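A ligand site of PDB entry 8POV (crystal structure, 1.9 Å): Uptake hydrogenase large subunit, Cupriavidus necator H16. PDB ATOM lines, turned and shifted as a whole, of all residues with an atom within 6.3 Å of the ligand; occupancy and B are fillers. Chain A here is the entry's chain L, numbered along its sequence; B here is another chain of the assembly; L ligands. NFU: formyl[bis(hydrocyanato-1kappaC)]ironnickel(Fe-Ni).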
ATOM      1  N   GLU A  27     -23.443  16.429  18.240  1.00  0.00           N
ATOM      2  CA  GLU A  27     -22.496  17.367  18.823  1.00  0.00           C
ATOM      3  C   GLU A  27     -22.181  16.866  20.236  1.00  0.00           C
ATOM      4  O   GLU A  27     -23.086  16.494  20.989  1.00  0.00           O
ATOM      5  CB  GLU A  27     -23.048  18.794  18.865  1.00  0.00           C
ATOM      6  CG  GLU A  27     -24.020  19.169  17.743  1.00  0.00           C
ATOM      7  CD  GLU A  27     -23.525  18.824  16.353  1.00  0.00           C
ATOM      8  OE1 GLU A  27     -22.291  18.661  16.140  1.00  0.00           O
ATOM      9  OE2 GLU A  27     -24.385  18.752  15.464  1.00  0.00           O
ATOM     10  N   ILE A  74     -20.737  27.600  25.002  1.00  0.00           N
ATOM     11  CA  ILE A  74     -21.395  26.345  25.364  1.00  0.00           C
ATOM     12  C   ILE A  74     -21.492  25.474  24.129  1.00  0.00           C
ATOM     13  O   ILE A  74     -21.369  24.265  24.219  1.00  0.00           O
ATOM     14  CB  ILE A  74     -22.798  26.556  25.966  1.00  0.00           C
ATOM     15  CG1 ILE A  74     -22.679  27.060  27.402  1.00  0.00           C
ATOM     16  CG2 ILE A  74     -23.611  25.260  25.932  1.00  0.00           C
ATOM     17  CD1 ILE A  74     -23.932  27.665  27.951  1.00  0.00           C
ATOM     18  N   CYS A  75     -21.719  26.106  22.980  1.00  0.00           N
ATOM     19  CA  CYS A  75     -21.917  25.341  21.738  1.00  0.00           C
ATOM     20  C   CYS A  75     -21.616  26.140  20.474  1.00  0.00           C
ATOM     21  O   CYS A  75     -22.143  27.209  20.274  1.00  0.00           O
ATOM     22  CB  CYS A  75     -23.354  24.837  21.682  1.00  0.00           C
ATOM     23  SG  CYS A  75     -23.623  23.755  20.281  1.00  0.00           S
ATOM     24  N   GLY A  76     -20.782  25.582  19.604  1.00  0.00           N
ATOM     25  CA  GLY A  76     -20.427  26.225  18.349  1.00  0.00           C
ATOM     26  C   GLY A  76     -21.300  25.822  17.168  1.00  0.00           C
ATOM     27  O   GLY A  76     -21.116  26.349  16.066  1.00  0.00           O
ATOM     28  N   VAL A  77     -22.243  24.902  17.397  1.00  0.00           N
ATOM     29  CA  VAL A  77     -23.195  24.470  16.369  1.00  0.00           C
ATOM     30  C   VAL A  77     -24.416  25.353  16.446  1.00  0.00           C
ATOM     31  O   VAL A  77     -24.786  25.978  15.449  1.00  0.00           O
ATOM     32  CB  VAL A  77     -23.625  22.987  16.558  1.00  0.00           C
ATOM     33  CG1 VAL A  77     -24.605  22.570  15.466  1.00  0.00           C
ATOM     34  CG2 VAL A  77     -22.404  22.081  16.544  1.00  0.00           C
ATOM     35  N   CYS A  78     -25.054  25.406  17.616  1.00  0.00           N
ATOM     36  CA  CYS A  78     -26.119  26.389  17.863  1.00  0.00           C
ATOM     37  C   CYS A  78     -25.481  27.684  18.362  1.00  0.00           C
ATOM     38  O   CYS A  78     -25.848  28.224  19.413  1.00  0.00           O
ATOM     39  CB  CYS A  78     -27.157  25.849  18.855  1.00  0.00           C
ATOM     40  SG  CYS A  78     -26.548  25.513  20.517  1.00  0.00           S
ATOM     41  N   THR A  79     -24.537  28.170  17.557  1.00  0.00           N
ATOM     42  CA  THR A  79     -23.680  29.289  17.935  1.00  0.00           C
ATOM     43  C   THR A  79     -24.432  30.611  17.869  1.00  0.00           C
ATOM     44  O   THR A  79     -24.939  30.996  16.811  1.00  0.00           O
ATOM     45  CB  THR A  79     -22.404  29.357  17.063  1.00  0.00           C
ATOM     46  OG1 THR A  79     -21.628  30.482  17.447  1.00  0.00           O
ATOM     47  CG2 THR A  79     -22.699  29.445  15.555  1.00  0.00           C
ATOM     48  N   CYS A  81     -27.136  31.363  19.811  1.00  0.00           N
ATOM     49  CA  CYS A  81     -28.418  31.257  20.505  1.00  0.00           C
ATOM     50  C   CYS A  81     -28.216  31.463  22.015  1.00  0.00           C
ATOM     51  O   CYS A  81     -29.078  32.034  22.690  1.00  0.00           O
ATOM     52  CB  CYS A  81     -29.140  29.938  20.187  1.00  0.00           C
ATOM     53  SG  CYS A  81     -28.501  28.454  20.990  1.00  0.00           S
ATOM     54  N   HIS A  82     -27.087  31.022  22.541  1.00  0.00           N
ATOM     55  CA  HIS A  82     -26.762  31.234  23.954  1.00  0.00           C
ATOM     56  C   HIS A  82     -26.412  32.694  24.221  1.00  0.00           C
ATOM     57  O   HIS A  82     -26.724  33.231  25.284  1.00  0.00           O
ATOM     58  CB  HIS A  82     -25.618  30.337  24.393  1.00  0.00           C
ATOM     59  CG  HIS A  82     -25.995  28.887  24.514  1.00  0.00           C
ATOM     60  ND1 HIS A  82     -26.795  28.407  25.524  1.00  0.00           N
ATOM     61  CD2 HIS A  82     -25.625  27.814  23.775  1.00  0.00           C
ATOM     62  CE1 HIS A  82     -26.939  27.096  25.384  1.00  0.00           C
ATOM     63  NE2 HIS A  82     -26.240  26.712  24.345  1.00  0.00           N
ATOM     64  N   ASP A 117     -28.193  25.416  10.878  1.00  0.00           N
ATOM     65  CA  ASP A 117     -28.116  24.321  11.830  1.00  0.00           C
ATOM     66  C   ASP A 117     -29.016  23.179  11.376  1.00  0.00           C
ATOM     67  O   ASP A 117     -28.591  22.037  11.326  1.00  0.00           O
ATOM     68  CB  ASP A 117     -28.534  24.842  13.207  1.00  0.00           C
ATOM     69  CG  ASP A 117     -28.011  24.013  14.345  1.00  0.00           C
ATOM     70  OD1 ASP A 117     -27.886  22.768  14.182  1.00  0.00           O
ATOM     71  OD2 ASP A 117     -27.766  24.599  15.425  1.00  0.00           O
ATOM     72  N   ALA A 528     -34.291  27.954  20.484  1.00  0.00           N
ATOM     73  CA  ALA A 528     -33.081  27.475  19.837  1.00  0.00           C
ATOM     74  C   ALA A 528     -33.428  26.345  18.848  1.00  0.00           C
ATOM     75  O   ALA A 528     -34.522  25.774  18.927  1.00  0.00           O
ATOM     76  CB  ALA A 528     -32.116  26.960  20.890  1.00  0.00           C
ATOM     77  N   PRO A 529     -32.506  26.023  17.931  1.00  0.00           N
ATOM     78  CA  PRO A 529     -32.781  24.993  16.938  1.00  0.00           C
ATOM     79  C   PRO A 529     -33.303  23.668  17.490  1.00  0.00           C
ATOM     80  O   PRO A 529     -34.094  23.016  16.828  1.00  0.00           O
ATOM     81  CB  PRO A 529     -31.418  24.807  16.264  1.00  0.00           C
ATOM     82  CG  PRO A 529     -30.823  26.174  16.315  1.00  0.00           C
ATOM     83  CD  PRO A 529     -31.241  26.733  17.636  1.00  0.00           C
ATOM     84  N   ARG A 530     -32.909  23.323  18.710  1.00  0.00           N
ATOM     85  CA  ARG A 530     -33.234  22.029  19.298  1.00  0.00           C
ATOM     86  C   ARG A 530     -34.397  22.085  20.284  1.00  0.00           C
ATOM     87  O   ARG A 530     -34.827  21.054  20.789  1.00  0.00           O
ATOM     88  CB  ARG A 530     -31.990  21.443  19.955  1.00  0.00           C
ATOM     89  CG  ARG A 530     -31.031  20.922  18.920  1.00  0.00           C
ATOM     90  CD  ARG A 530     -29.591  20.887  19.383  1.00  0.00           C
ATOM     91  NE  ARG A 530     -28.719  20.543  18.263  1.00  0.00           N
ATOM     92  CZ  ARG A 530     -28.292  21.413  17.336  1.00  0.00           C
ATOM     93  NH1 ARG A 530     -28.627  22.690  17.407  1.00  0.00           N
ATOM     94  NH2 ARG A 530     -27.512  20.984  16.347  1.00  0.00           N
ATOM     95  N   GLY A 531     -34.913  23.296  20.534  1.00  0.00           N
ATOM     96  CA  GLY A 531     -36.086  23.472  21.398  1.00  0.00           C
ATOM     97  C   GLY A 531     -35.970  24.665  22.299  1.00  0.00           C
ATOM     98  O   GLY A 531     -35.420  25.705  21.911  1.00  0.00           O
ATOM     99  N   ALA A 532     -36.447  24.507  23.538  1.00  0.00           N
ATOM    100  CA  ALA A 532     -36.627  25.587  24.475  1.00  0.00           C
ATOM    101  C   ALA A 532     -35.369  25.871  25.290  1.00  0.00           C
ATOM    102  O   ALA A 532     -34.944  25.048  26.115  1.00  0.00           O
ATOM    103  CB  ALA A 532     -37.802  25.269  25.387  1.00  0.00           C
ATOM    104  N   LEU A 533     -34.774  27.049  25.061  1.00  0.00           N
ATOM    105  CA  LEU A 533     -33.578  27.481  25.770  1.00  0.00           C
ATOM    106  C   LEU A 533     -33.907  28.612  26.732  1.00  0.00           C
ATOM    107  O   LEU A 533     -34.588  29.574  26.350  1.00  0.00           O
ATOM    108  CB  LEU A 533     -32.498  27.972  24.806  1.00  0.00           C
ATOM    109  CG  LEU A 533     -31.244  28.647  25.408  1.00  0.00           C
ATOM    110  CD1 LEU A 533     -30.476  27.685  26.321  1.00  0.00           C
ATOM    111  CD2 LEU A 533     -30.316  29.192  24.326  1.00  0.00           C
ATOM    112  N   VAL A 550     -30.889  26.241  31.201  1.00  0.00           N
ATOM    113  CA  VAL A 550     -31.657  25.026  30.888  1.00  0.00           C
ATOM    114  C   VAL A 550     -31.849  25.016  29.382  1.00  0.00           C
ATOM    115  O   VAL A 550     -32.440  25.925  28.807  1.00  0.00           O
ATOM    116  CB  VAL A 550     -33.004  24.967  31.625  1.00  0.00           C
ATOM    117  CG1 VAL A 550     -33.678  23.635  31.382  1.00  0.00           C
ATOM    118  CG2 VAL A 550     -32.798  25.175  33.118  1.00  0.00           C
ATOM    119  N   VAL A 551     -31.306  23.987  28.757  1.00  0.00           N
ATOM    120  CA  VAL A 551     -31.002  23.996  27.340  1.00  0.00           C
ATOM    121  C   VAL A 551     -31.829  22.871  26.690  1.00  0.00           C
ATOM    122  O   VAL A 551     -32.206  21.927  27.371  1.00  0.00           O
ATOM    123  CB  VAL A 551     -29.466  23.838  27.172  1.00  0.00           C
ATOM    124  CG1 VAL A 551     -29.033  24.025  25.742  1.00  0.00           C
ATOM    125  CG2 VAL A 551     -28.744  24.881  28.016  1.00  0.00           C
ATOM    126  N   PRO A 552     -32.160  23.001  25.392  1.00  0.00           N
ATOM    127  CA  PRO A 552     -33.156  22.054  24.863  1.00  0.00           C
ATOM    128  C   PRO A 552     -32.773  20.608  25.024  1.00  0.00           C
ATOM    129  O   PRO A 552     -33.620  19.779  25.367  1.00  0.00           O
ATOM    130  CB  PRO A 552     -33.253  22.436  23.386  1.00  0.00           C
ATOM    131  CG  PRO A 552     -32.842  23.873  23.337  1.00  0.00           C
ATOM    132  CD  PRO A 552     -31.870  24.079  24.443  1.00  0.00           C
ATOM    133  N   THR A 553     -31.514  20.290  24.790  1.00  0.00           N
ATOM    134  CA  THR A 553     -31.056  18.920  24.862  1.00  0.00           C
ATOM    135  C   THR A 553     -31.012  18.471  26.327  1.00  0.00           C
ATOM    136  O   THR A 553     -31.152  17.281  26.597  1.00  0.00           O
ATOM    137  CB  THR A 553     -29.742  18.708  24.103  1.00  0.00           C
ATOM    138  OG1 THR A 553     -29.939  19.063  22.714  1.00  0.00           O
ATOM    139  CG2 THR A 553     -29.303  17.248  24.175  1.00  0.00           C
ATOM    140  N   THR A 554     -30.866  19.424  27.265  1.00  0.00           N
ATOM    141  CA  THR A 554     -31.088  19.116  28.690  1.00  0.00           C
ATOM    142  C   THR A 554     -32.497  18.511  28.879  1.00  0.00           C
ATOM    143  O   THR A 554     -32.650  17.474  29.506  1.00  0.00           O
ATOM    144  CB  THR A 554     -30.938  20.334  29.607  1.00  0.00           C
ATOM    145  OG1 THR A 554     -29.821  21.141  29.187  1.00  0.00           O
ATOM    146  CG2 THR A 554     -30.736  19.894  31.054  1.00  0.00           C
ATOM    147  N   ASP A 595     -31.665  15.821  17.028  1.00  0.00           N
ATOM    148  CA  ASP A 595     -30.491  16.678  16.822  1.00  0.00           C
ATOM    149  C   ASP A 595     -29.765  16.921  18.167  1.00  0.00           C
ATOM    150  O   ASP A 595     -29.668  18.055  18.643  1.00  0.00           O
ATOM    151  CB  ASP A 595     -30.939  17.994  16.193  1.00  0.00           C
ATOM    152  CG  ASP A 595     -29.794  18.829  15.687  1.00  0.00           C
ATOM    153  OD1 ASP A 595     -28.610  18.449  15.840  1.00  0.00           O
ATOM    154  OD2 ASP A 595     -30.074  19.907  15.121  1.00  0.00           O
ATOM    155  N   PRO A 596     -29.281  15.838  18.790  1.00  0.00           N
ATOM    156  CA  PRO A 596     -28.689  15.971  20.125  1.00  0.00           C
ATOM    157  C   PRO A 596     -27.458  16.870  20.161  1.00  0.00           C
ATOM    158  O   PRO A 596     -26.502  16.648  19.416  1.00  0.00           O
ATOM    159  CB  PRO A 596     -28.321  14.521  20.485  1.00  0.00           C
ATOM    160  CG  PRO A 596     -29.227  13.686  19.642  1.00  0.00           C
ATOM    161  CD  PRO A 596     -29.324  14.430  18.360  1.00  0.00           C
ATOM    162  N   CYS A 597     -27.495  17.902  20.995  1.00  0.00           N
ATOM    163  CA  CYS A 597     -26.336  18.737  21.246  1.00  0.00           C
ATOM    164  C   CYS A 597     -25.921  18.518  22.703  1.00  0.00           C
ATOM    165  O   CYS A 597     -26.527  19.076  23.625  1.00  0.00           O
ATOM    166  CB  CYS A 597     -26.632  20.202  20.958  1.00  0.00           C
ATOM    167  SG  CYS A 597     -25.167  21.261  20.961  1.00  0.00           S
ATOM    168  N   LEU A 598     -24.917  17.688  22.903  1.00  0.00           N
ATOM    169  CA  LEU A 598     -24.595  17.221  24.256  1.00  0.00           C
ATOM    170  C   LEU A 598     -23.784  18.229  25.046  1.00  0.00           C
ATOM    171  O   LEU A 598     -23.894  18.292  26.258  1.00  0.00           O
ATOM    172  CB  LEU A 598     -23.856  15.874  24.210  1.00  0.00           C
ATOM    173  CG  LEU A 598     -24.800  14.684  24.074  1.00  0.00           C
ATOM    174  CD1 LEU A 598     -25.570  14.424  25.367  1.00  0.00           C
ATOM    175  CD2 LEU A 598     -25.765  14.863  22.935  1.00  0.00           C
ATOM    176  N   ALA A 599     -22.999  19.050  24.357  1.00  0.00           N
ATOM    177  CA  ALA A 599     -22.267  20.109  25.027  1.00  0.00           C
ATOM    178  C   ALA A 599     -23.271  21.130  25.571  1.00  0.00           C
ATOM    179  O   ALA A 599     -23.180  21.575  26.722  1.00  0.00           O
ATOM    180  CB  ALA A 599     -21.262  20.737  24.077  1.00  0.00           C
ATOM    181  N   CYS A 600     -24.265  21.452  24.766  1.00  0.00           N
ATOM    182  CA  CYS A 600     -25.417  22.220  25.222  1.00  0.00           C
ATOM    183  C   CYS A 600     -26.084  21.646  26.462  1.00  0.00           C
ATOM    184  O   CYS A 600     -26.348  22.373  27.423  1.00  0.00           O
ATOM    185  CB  CYS A 600     -26.453  22.316  24.119  1.00  0.00           C
ATOM    186  SG  CYS A 600     -26.337  23.846  23.222  1.00  0.00           S
ATOM    187  N   SER A 601     -26.372  20.342  26.415  1.00  0.00           N
ATOM    188  CA  SER A 601     -27.198  19.714  27.440  1.00  0.00           C
ATOM    189  C   SER A 601     -26.572  19.842  28.818  1.00  0.00           C
ATOM    190  O   SER A 601     -27.271  19.963  29.819  1.00  0.00           O
ATOM    191  CB  SER A 601     -27.462  18.250  27.110  1.00  0.00           C
ATOM    192  OG  SER A 601     -26.273  17.448  27.169  1.00  0.00           O
ATOM    193  N   CYS B  17     -16.879  22.749  22.367  1.00  0.00           N
ATOM    194  CA  CYS B  17     -18.183  23.214  21.952  1.00  0.00           C
ATOM    195  C   CYS B  17     -18.475  22.827  20.506  1.00  0.00           C
ATOM    196  O   CYS B  17     -19.560  23.101  20.003  1.00  0.00           O
ATOM    197  CB  CYS B  17     -18.281  24.711  22.121  1.00  0.00           C
ATOM    198  SG  CYS B  17     -17.634  25.646  20.734  1.00  0.00           S
HETATM  199 FE   NFU L   1     -28.013  24.007  21.654  1.00  0.00          FE
HETATM  200 NI   NFU L   1     -25.775  23.208  20.631  1.00  0.00          NI
HETATM  201  C1  NFU L   1     -29.458  24.191  20.390  1.00  0.00           C
HETATM  202  N1  NFU L   1     -30.315  24.315  19.668  1.00  0.00           N
HETATM  203  C2  NFU L   1     -29.158  22.627  22.387  1.00  0.00           C
HETATM  204  N2  NFU L   1     -29.796  21.822  22.838  1.00  0.00           N
HETATM  205  C3  NFU L   1     -28.994  25.279  22.619  1.00  0.00           C
HETATM  206  O3  NFU L   1     -29.582  26.127  23.234  1.00  0.00           O
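N of Thr 553 lies within hydrogen-bond range of N2 of the ligand. N1 of the ligand sits at hydrogen-bond distance from N of Arg 530, at 2.9 Å. An iron atom (FE) of the ligand is bound by the side-chain sulfur (SG) of Cys 600 (2.3 Å). SG of Cys 75 binds NI of the ligand (2.2 Å). SG of Cys 597 is bound to NI of the ligand, 2.1 Å away. N1 of the ligand sits at hydrogen-bond distance from NH1 of Arg 530, at 3.3 Å. The side-chain hydroxyl of Thr 553 sits at hydrogen-bond distance from a nitrogen (N2) of the ligand. An iron atom (FE) of the ligand is bound by the side-chain sulfur (SG) of Cys 78 (2.4 Å). An oxygen (O3) of the ligand is in hydrogen-bond range of the side-chain sulfur of Cys 81 (3.4 Å).
The side-chain carboxylate of Asp 595 lies within salt-bridge range of the guanidinium group of Arg 530. The side-chain carboxylate (OD1) of Asp 117 is in salt-bridge range of the guanidinium group (NH2) of Arg 530, at 2.8 Å. The side-chain sulfur of Cys 600 sits close to a ring nitrogen (NE2) of His 82, at 3.1 Å. The side-chain carboxylate of Glu 27 is in salt-bridge range of the guanidinium group of Arg 530 (3.9 Å). OG1 of Thr 553 lies within hydrogen-bond range of N of Cys 597, 3.2 Å away. SG of Cys 75 lies close to N of Val 77 (3.4 Å). The backbone carbonyl oxygen (O) of Cys 78 lies within hydrogen-bond range of the side-chain sulfur (SG) of Cys 81 (3.1 Å). The backbone carbonyl oxygen (O) of Val 551 lies close to the side-chain hydroxyl (OG1) of Thr 554, at 3.1 Å.
N of Pro 529 sits close to N1 of the ligand (3.3 Å). CE1 of His 82 touches O3 of the ligand (3.5 Å). CB of Ala 528 touches N1 of the ligand, at 3.4 Å. Leu 533 touches the ligand. Val 551 touches the ligand (CG1 to O3, 3.3 Å). CD of Pro 552 touches O3 of the ligand, 3.3 Å away. Hydrophobic or aromatic side chains that line the ligand: His 82, Ala 528, Pro 529, Leu 533, Val 551 and Pro 552. Within 4 Å of the ligand: Cys 75, Cys 78, Cys 81, His 82, Ala 528, Pro 529, Arg 530, Leu 533, Val 551, Pro 552, Thr 553, Cys 597 and Cys 600.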
